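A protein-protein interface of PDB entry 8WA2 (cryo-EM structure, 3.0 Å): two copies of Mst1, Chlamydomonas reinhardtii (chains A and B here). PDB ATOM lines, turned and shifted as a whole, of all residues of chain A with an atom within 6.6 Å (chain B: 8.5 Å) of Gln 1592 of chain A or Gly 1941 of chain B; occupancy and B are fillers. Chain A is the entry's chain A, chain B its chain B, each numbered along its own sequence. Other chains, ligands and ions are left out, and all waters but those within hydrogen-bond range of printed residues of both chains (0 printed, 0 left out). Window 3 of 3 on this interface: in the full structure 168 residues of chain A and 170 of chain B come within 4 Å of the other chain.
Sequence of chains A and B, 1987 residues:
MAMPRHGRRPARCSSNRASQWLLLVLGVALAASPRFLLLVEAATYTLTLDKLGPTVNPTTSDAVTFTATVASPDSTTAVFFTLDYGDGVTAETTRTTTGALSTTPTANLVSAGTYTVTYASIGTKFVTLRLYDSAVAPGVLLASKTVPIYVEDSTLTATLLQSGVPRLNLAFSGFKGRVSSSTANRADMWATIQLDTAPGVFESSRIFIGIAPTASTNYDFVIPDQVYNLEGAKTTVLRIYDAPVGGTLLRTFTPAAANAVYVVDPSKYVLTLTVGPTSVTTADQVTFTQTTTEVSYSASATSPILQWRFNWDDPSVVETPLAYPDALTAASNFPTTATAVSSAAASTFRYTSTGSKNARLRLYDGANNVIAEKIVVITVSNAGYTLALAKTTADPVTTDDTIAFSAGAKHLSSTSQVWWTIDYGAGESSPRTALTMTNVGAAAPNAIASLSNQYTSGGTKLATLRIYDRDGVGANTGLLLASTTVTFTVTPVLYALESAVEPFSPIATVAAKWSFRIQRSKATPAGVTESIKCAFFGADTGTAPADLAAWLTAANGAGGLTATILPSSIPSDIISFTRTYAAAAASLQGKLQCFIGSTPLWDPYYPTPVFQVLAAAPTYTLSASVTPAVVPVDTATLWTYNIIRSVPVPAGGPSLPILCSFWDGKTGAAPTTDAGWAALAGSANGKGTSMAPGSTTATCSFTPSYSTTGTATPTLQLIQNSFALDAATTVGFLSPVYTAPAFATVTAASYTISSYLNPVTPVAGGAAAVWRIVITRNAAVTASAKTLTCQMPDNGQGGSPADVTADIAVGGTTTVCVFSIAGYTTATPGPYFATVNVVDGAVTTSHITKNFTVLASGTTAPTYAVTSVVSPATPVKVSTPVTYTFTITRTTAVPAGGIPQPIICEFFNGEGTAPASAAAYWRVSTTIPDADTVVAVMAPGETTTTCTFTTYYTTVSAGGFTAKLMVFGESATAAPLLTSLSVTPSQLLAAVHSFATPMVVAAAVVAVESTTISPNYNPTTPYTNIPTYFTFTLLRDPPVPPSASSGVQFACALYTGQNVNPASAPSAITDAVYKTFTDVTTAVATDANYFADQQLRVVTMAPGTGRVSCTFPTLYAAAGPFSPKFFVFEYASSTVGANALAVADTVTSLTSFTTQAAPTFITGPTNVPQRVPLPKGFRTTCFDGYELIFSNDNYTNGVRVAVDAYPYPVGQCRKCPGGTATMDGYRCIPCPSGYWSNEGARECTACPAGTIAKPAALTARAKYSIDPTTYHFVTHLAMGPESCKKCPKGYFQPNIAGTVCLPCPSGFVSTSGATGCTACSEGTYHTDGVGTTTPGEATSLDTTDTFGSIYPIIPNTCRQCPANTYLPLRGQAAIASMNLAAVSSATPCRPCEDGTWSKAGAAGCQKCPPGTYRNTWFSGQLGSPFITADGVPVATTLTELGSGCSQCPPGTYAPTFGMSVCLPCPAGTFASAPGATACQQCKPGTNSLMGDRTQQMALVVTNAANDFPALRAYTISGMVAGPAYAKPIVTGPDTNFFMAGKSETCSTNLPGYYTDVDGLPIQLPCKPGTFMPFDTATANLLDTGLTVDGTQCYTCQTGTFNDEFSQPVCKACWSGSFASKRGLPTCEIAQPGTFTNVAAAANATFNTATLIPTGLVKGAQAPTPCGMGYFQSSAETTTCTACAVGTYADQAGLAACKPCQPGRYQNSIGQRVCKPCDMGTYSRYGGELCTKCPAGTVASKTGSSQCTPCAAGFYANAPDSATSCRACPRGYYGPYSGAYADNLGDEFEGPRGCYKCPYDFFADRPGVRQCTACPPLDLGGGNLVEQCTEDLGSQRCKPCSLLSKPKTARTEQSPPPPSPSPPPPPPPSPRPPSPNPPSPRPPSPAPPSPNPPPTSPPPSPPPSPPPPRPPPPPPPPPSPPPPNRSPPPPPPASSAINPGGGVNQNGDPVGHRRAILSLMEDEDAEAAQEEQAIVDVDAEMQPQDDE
The backbone NH (N) of Phe 1571 of chain A sits at hydrogen-bond distance from the backbone carbonyl oxygen (O) of Tyr 1594 of chain A, 2.8 Å away. The side-chain sulfur of Cys 1566 of chain A is disulfide-bonded to the side-chain sulfur of Cys 1593 of chain A (2.0 Å).
Among the printed residues, merely in contact across the chains: Phe 1571 of chain A with Asn 1944 of chain B (3.6 Å), Gln 1592 of chain A with Gly 1941 of chain B (3.8 Å), Gln 1592 of chain A with Gly 1942 of chain B (3.8 Å), Cys 1593 of chain A with Gly 1942 of chain B (3.9 Å) and Tyr 1594 of chain A with Gly 1942 of chain B (3.7 Å).
Of the printed residues of chain B, Phe 1571 of chain A touches Asn 1944 (3.6 Å). Thr 1587 of chain A touches none of the printed residues of chain B. Of the printed residues of chain B, Gln 1592 of chain A touches Gly 1941 (3.8 Å) and Gly 1942 (3.8 Å). Cys 1593 of chain A touches just one residue of chain B: Gly 1942 (3.9 Å). Pro 1939 of chain B touches none of the printed residues of chain A. Printed residues of chain A within 4 Å of Gly 1942 of chain B: Gln 1592 (3.8 Å), Cys 1593 (3.9 Å) and Tyr 1594 (3.7 Å). The nearest residue of chain A that does not touch Gly 1941 of chain B is Tyr 1594 of chain A (5.4 Å).
Hydrophobic or aromatic side chains of chain A within 4 Å of the printed part of chain B: Phe 1571 and Tyr 1594. Among the printed residues, 5 pairs touch across the chains. Among the printed residues, no Asp or Glu carboxylate lies within 4 Å of a Lys or Arg side-chain nitrogen of the other chain.
No position is printed for both chains.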
ATOM      1  N   TYR A1554       1.603 -34.603  11.885  1.00  0.00           N
ATOM      2  CA  TYR A1554       1.267 -33.326  12.498  1.00  0.00           C
ATOM      3  C   TYR A1554       0.658 -33.552  13.873  1.00  0.00           C
ATOM      4  O   TYR A1554       0.081 -34.606  14.147  1.00  0.00           O
ATOM      5  CB  TYR A1554       0.287 -32.531  11.632  1.00  0.00           C
ATOM      6  CG  TYR A1554      -1.131 -33.052  11.652  1.00  0.00           C
ATOM      7  CD1 TYR A1554      -1.504 -34.131  10.874  1.00  0.00           C
ATOM      8  CD2 TYR A1554      -2.104 -32.443  12.427  1.00  0.00           C
ATOM      9  CE1 TYR A1554      -2.798 -34.603  10.879  1.00  0.00           C
ATOM     10  CE2 TYR A1554      -3.400 -32.910  12.440  1.00  0.00           C
ATOM     11  CZ  TYR A1554      -3.741 -33.990  11.663  1.00  0.00           C
ATOM     12  OH  TYR A1554      -5.032 -34.462  11.667  1.00  0.00           O
ATOM     13  N   THR A1555       0.791 -32.541  14.732  1.00  0.00           N
ATOM     14  CA  THR A1555       0.106 -32.494  16.020  1.00  0.00           C
ATOM     15  C   THR A1555      -0.422 -31.083  16.216  1.00  0.00           C
ATOM     16  O   THR A1555       0.360 -30.128  16.231  1.00  0.00           O
ATOM     17  CB  THR A1555       1.036 -32.870  17.177  1.00  0.00           C
ATOM     18  OG1 THR A1555       2.233 -32.087  17.100  1.00  0.00           O
ATOM     19  CG2 THR A1555       1.395 -34.342  17.124  1.00  0.00           C
ATOM     20  N   ASP A1556      -1.738 -30.949  16.378  1.00  0.00           N
ATOM     21  CA  ASP A1556      -2.361 -29.634  16.442  1.00  0.00           C
ATOM     22  C   ASP A1556      -2.728 -29.190  17.850  1.00  0.00           C
ATOM     23  O   ASP A1556      -2.942 -27.992  18.063  1.00  0.00           O
ATOM     24  CB  ASP A1556      -3.622 -29.602  15.572  1.00  0.00           C
ATOM     25  CG  ASP A1556      -4.330 -30.937  15.528  1.00  0.00           C
ATOM     26  OD1 ASP A1556      -4.043 -31.794  16.389  1.00  0.00           O
ATOM     27  OD2 ASP A1556      -5.180 -31.131  14.635  1.00  0.00           O
ATOM     28  N   CYS A1566      -0.990 -37.178   7.888  1.00  0.00           N
ATOM     29  CA  CYS A1566      -1.783 -36.343   6.998  1.00  0.00           C
ATOM     30  C   CYS A1566      -2.724 -37.209   6.168  1.00  0.00           C
ATOM     31  O   CYS A1566      -2.347 -38.277   5.682  1.00  0.00           O
ATOM     32  CB  CYS A1566      -0.878 -35.520   6.082  1.00  0.00           C
ATOM     33  SG  CYS A1566      -0.056 -34.096   6.854  1.00  0.00           S
ATOM     34  N   PHE A1571      -0.623 -33.065   2.432  1.00  0.00           N
ATOM     35  CA  PHE A1571       0.772 -33.454   2.592  1.00  0.00           C
ATOM     36  C   PHE A1571       1.432 -32.536   3.611  1.00  0.00           C
ATOM     37  O   PHE A1571       0.900 -31.484   3.970  1.00  0.00           O
ATOM     38  CB  PHE A1571       1.521 -33.423   1.257  1.00  0.00           C
ATOM     39  CG  PHE A1571       1.962 -32.053   0.836  1.00  0.00           C
ATOM     40  CD1 PHE A1571       1.042 -31.123   0.391  1.00  0.00           C
ATOM     41  CD2 PHE A1571       3.297 -31.697   0.878  1.00  0.00           C
ATOM     42  CE1 PHE A1571       1.444 -29.868  -0.001  1.00  0.00           C
ATOM     43  CE2 PHE A1571       3.703 -30.441   0.488  1.00  0.00           C
ATOM     44  CZ  PHE A1571       2.775 -29.527   0.049  1.00  0.00           C
ATOM     45  N   MET A1572       2.606 -32.955   4.076  1.00  0.00           N
ATOM     46  CA  MET A1572       3.419 -32.202   5.025  1.00  0.00           C
ATOM     47  C   MET A1572       4.896 -32.308   4.670  1.00  0.00           C
ATOM     48  O   MET A1572       5.500 -33.375   4.835  1.00  0.00           O
ATOM     49  CB  MET A1572       3.197 -32.696   6.453  1.00  0.00           C
ATOM     50  CG  MET A1572       3.986 -31.917   7.496  1.00  0.00           C
ATOM     51  SD  MET A1572       3.282 -30.324   7.937  1.00  0.00           S
ATOM     52  CE  MET A1572       2.088 -30.831   9.163  1.00  0.00           C
ATOM     53  N   PRO A1573       5.512 -31.234   4.190  1.00  0.00           N
ATOM     54  CA  PRO A1573       6.928 -31.305   3.804  1.00  0.00           C
ATOM     55  C   PRO A1573       7.872 -31.348   4.994  1.00  0.00           C
ATOM     56  O   PRO A1573       7.436 -31.262   6.145  1.00  0.00           O
ATOM     57  CB  PRO A1573       7.128 -30.027   2.986  1.00  0.00           C
ATOM     58  CG  PRO A1573       6.105 -29.093   3.504  1.00  0.00           C
ATOM     59  CD  PRO A1573       4.922 -29.917   3.900  1.00  0.00           C
ATOM     60  N   THR A1587       3.865 -21.141   5.259  1.00  0.00           N
ATOM     61  CA  THR A1587       4.957 -21.704   6.035  1.00  0.00           C
ATOM     62  C   THR A1587       4.482 -22.985   6.702  1.00  0.00           C
ATOM     63  O   THR A1587       3.301 -23.131   7.027  1.00  0.00           O
ATOM     64  CB  THR A1587       5.459 -20.734   7.108  1.00  0.00           C
ATOM     65  OG1 THR A1587       4.556 -20.745   8.221  1.00  0.00           O
ATOM     66  CG2 THR A1587       5.552 -19.324   6.555  1.00  0.00           C
ATOM     67  N   VAL A1588       5.411 -23.912   6.910  1.00  0.00           N
ATOM     68  CA  VAL A1588       5.112 -25.203   7.517  1.00  0.00           C
ATOM     69  C   VAL A1588       5.816 -25.277   8.862  1.00  0.00           C
ATOM     70  O   VAL A1588       7.029 -25.057   8.951  1.00  0.00           O
ATOM     71  CB  VAL A1588       5.528 -26.368   6.605  1.00  0.00           C
ATOM     72  CG1 VAL A1588       6.857 -26.084   5.963  1.00  0.00           C
ATOM     73  CG2 VAL A1588       5.596 -27.657   7.396  1.00  0.00           C
ATOM     74  N   ASP A1589       5.050 -25.583   9.909  1.00  0.00           N
ATOM     75  CA  ASP A1589       5.579 -25.667  11.260  1.00  0.00           C
ATOM     76  C   ASP A1589       5.258 -26.984  11.950  1.00  0.00           C
ATOM     77  O   ASP A1589       5.669 -27.173  13.099  1.00  0.00           O
ATOM     78  CB  ASP A1589       5.048 -24.507  12.113  1.00  0.00           C
ATOM     79  CG  ASP A1589       3.581 -24.230  11.863  1.00  0.00           C
ATOM     80  OD1 ASP A1589       3.013 -24.828  10.927  1.00  0.00           O
ATOM     81  OD2 ASP A1589       2.995 -23.411  12.598  1.00  0.00           O
ATOM     82  N   GLY A1590       4.543 -27.891  11.294  1.00  0.00           N
ATOM     83  CA  GLY A1590       4.222 -29.177  11.869  1.00  0.00           C
ATOM     84  C   GLY A1590       2.829 -29.314  12.437  1.00  0.00           C
ATOM     85  O   GLY A1590       2.527 -30.350  13.038  1.00  0.00           O
ATOM     86  N   THR A1591       1.971 -28.307  12.272  1.00  0.00           N
ATOM     87  CA  THR A1591       0.616 -28.357  12.798  1.00  0.00           C
ATOM     88  C   THR A1591      -0.464 -28.404  11.729  1.00  0.00           C
ATOM     89  O   THR A1591      -1.608 -28.732  12.050  1.00  0.00           O
ATOM     90  CB  THR A1591       0.349 -27.149  13.706  1.00  0.00           C
ATOM     91  OG1 THR A1591       0.194 -25.974  12.903  1.00  0.00           O
ATOM     92  CG2 THR A1591       1.499 -26.945  14.666  1.00  0.00           C
ATOM     93  N   GLN A1592      -0.137 -28.090  10.478  1.00  0.00           N
ATOM     94  CA  GLN A1592      -1.129 -28.010   9.415  1.00  0.00           C
ATOM     95  C   GLN A1592      -0.681 -28.844   8.229  1.00  0.00           C
ATOM     96  O   GLN A1592       0.429 -28.659   7.724  1.00  0.00           O
ATOM     97  CB  GLN A1592      -1.340 -26.559   8.978  1.00  0.00           C
ATOM     98  CG  GLN A1592      -2.573 -25.910   9.550  1.00  0.00           C
ATOM     99  CD  GLN A1592      -2.650 -24.443   9.207  1.00  0.00           C
ATOM    100  OE1 GLN A1592      -1.659 -23.840   8.798  1.00  0.00           O
ATOM    101  NE2 GLN A1592      -3.828 -23.858   9.371  1.00  0.00           N
ATOM    102  N   CYS A1593      -1.547 -29.749   7.780  1.00  0.00           N
ATOM    103  CA  CYS A1593      -1.354 -30.429   6.508  1.00  0.00           C
ATOM    104  C   CYS A1593      -1.909 -29.543   5.400  1.00  0.00           C
ATOM    105  O   CYS A1593      -3.035 -29.047   5.503  1.00  0.00           O
ATOM    106  CB  CYS A1593      -2.047 -31.794   6.483  1.00  0.00           C
ATOM    107  SG  CYS A1593      -1.527 -32.999   7.732  1.00  0.00           S
ATOM    108  N   TYR A1594      -1.122 -29.345   4.350  1.00  0.00           N
ATOM    109  CA  TYR A1594      -1.524 -28.511   3.229  1.00  0.00           C
ATOM    110  C   TYR A1594      -2.090 -29.368   2.105  1.00  0.00           C
ATOM    111  O   TYR A1594      -1.654 -30.499   1.884  1.00  0.00           O
ATOM    112  CB  TYR A1594      -0.345 -27.690   2.707  1.00  0.00           C
ATOM    113  CG  TYR A1594       0.089 -26.589   3.642  1.00  0.00           C
ATOM    114  CD1 TYR A1594      -0.514 -25.343   3.600  1.00  0.00           C
ATOM    115  CD2 TYR A1594       1.103 -26.791   4.562  1.00  0.00           C
ATOM    116  CE1 TYR A1594      -0.125 -24.335   4.449  1.00  0.00           C
ATOM    117  CE2 TYR A1594       1.500 -25.787   5.416  1.00  0.00           C
ATOM    118  CZ  TYR A1594       0.881 -24.562   5.354  1.00  0.00           C
ATOM    119  OH  TYR A1594       1.273 -23.557   6.202  1.00  0.00           O
ATOM    120  N   ILE B1937      -9.324 -17.684  13.620  1.00  0.00           N
ATOM    121  CA  ILE B1937      -8.008 -17.744  13.004  1.00  0.00           C
ATOM    122  C   ILE B1937      -8.068 -17.166  11.594  1.00  0.00           C
ATOM    123  O   ILE B1937      -9.136 -17.024  10.987  1.00  0.00           O
ATOM    124  CB  ILE B1937      -7.472 -19.184  12.999  1.00  0.00           C
ATOM    125  CG1 ILE B1937      -8.367 -20.086  12.156  1.00  0.00           C
ATOM    126  CG2 ILE B1937      -7.369 -19.716  14.413  1.00  0.00           C
ATOM    127  CD1 ILE B1937      -7.938 -21.529  12.162  1.00  0.00           C
ATOM    128  N   ASN B1938      -6.896 -16.820  11.071  1.00  0.00           N
ATOM    129  CA  ASN B1938      -6.827 -16.161   9.777  1.00  0.00           C
ATOM    130  C   ASN B1938      -7.360 -17.085   8.685  1.00  0.00           C
ATOM    131  O   ASN B1938      -7.112 -18.296   8.720  1.00  0.00           O
ATOM    132  CB  ASN B1938      -5.390 -15.748   9.460  1.00  0.00           C
ATOM    133  CG  ASN B1938      -4.736 -15.009  10.602  1.00  0.00           C
ATOM    134  OD1 ASN B1938      -4.343 -15.610  11.601  1.00  0.00           O
ATOM    135  ND2 ASN B1938      -4.624 -13.694  10.468  1.00  0.00           N
ATOM    136  N   PRO B1939      -8.082 -16.553   7.705  1.00  0.00           N
ATOM    137  CA  PRO B1939      -8.705 -17.412   6.694  1.00  0.00           C
ATOM    138  C   PRO B1939      -7.682 -17.993   5.733  1.00  0.00           C
ATOM    139  O   PRO B1939      -6.546 -17.527   5.620  1.00  0.00           O
ATOM    140  CB  PRO B1939      -9.673 -16.471   5.966  1.00  0.00           C
ATOM    141  CG  PRO B1939      -9.680 -15.193   6.753  1.00  0.00           C
ATOM    142  CD  PRO B1939      -8.386 -15.133   7.480  1.00  0.00           C
ATOM    143  N   GLY B1940      -8.115 -19.030   5.024  1.00  0.00           N
ATOM    144  CA  GLY B1940      -7.260 -19.701   4.062  1.00  0.00           C
ATOM    145  C   GLY B1940      -6.108 -20.457   4.681  1.00  0.00           C
ATOM    146  O   GLY B1940      -5.003 -20.462   4.123  1.00  0.00           O
ATOM    147  N   GLY B1941      -6.336 -21.102   5.824  1.00  0.00           N
ATOM    148  CA  GLY B1941      -5.296 -21.868   6.481  1.00  0.00           C
ATOM    149  C   GLY B1941      -5.250 -23.284   5.946  1.00  0.00           C
ATOM    150  O   GLY B1941      -6.274 -23.968   5.886  1.00  0.00           O
ATOM    151  N   GLY B1942      -4.055 -23.720   5.563  1.00  0.00           N
ATOM    152  CA  GLY B1942      -3.895 -25.056   5.028  1.00  0.00           C
ATOM    153  C   GLY B1942      -4.426 -25.241   3.629  1.00  0.00           C
ATOM    154  O   GLY B1942      -4.697 -26.374   3.226  1.00  0.00           O
ATOM    155  N   VAL B1943      -4.585 -24.159   2.876  1.00  0.00           N
ATOM    156  CA  VAL B1943      -5.048 -24.205   1.496  1.00  0.00           C
ATOM    157  C   VAL B1943      -3.856 -23.876   0.613  1.00  0.00           C
ATOM    158  O   VAL B1943      -3.322 -22.761   0.666  1.00  0.00           O
ATOM    159  CB  VAL B1943      -6.207 -23.232   1.247  1.00  0.00           C
ATOM    160  CG1 VAL B1943      -6.407 -23.016  -0.240  1.00  0.00           C
ATOM    161  CG2 VAL B1943      -7.476 -23.758   1.876  1.00  0.00           C
ATOM    162  N   ASN B1944      -3.438 -24.840  -0.200  1.00  0.00           N
ATOM    163  CA  ASN B1944      -2.289 -24.651  -1.066  1.00  0.00           C
ATOM    164  C   ASN B1944      -2.714 -23.996  -2.374  1.00  0.00           C
ATOM    165  O   ASN B1944      -3.901 -23.848  -2.670  1.00  0.00           O
ATOM    166  CB  ASN B1944      -1.596 -25.982  -1.338  1.00  0.00           C
ATOM    167  CG  ASN B1944      -0.117 -25.824  -1.576  1.00  0.00           C
ATOM    168  OD1 ASN B1944       0.418 -24.721  -1.495  1.00  0.00           O
ATOM    169  ND2 ASN B1944       0.558 -26.926  -1.872  1.00  0.00           N
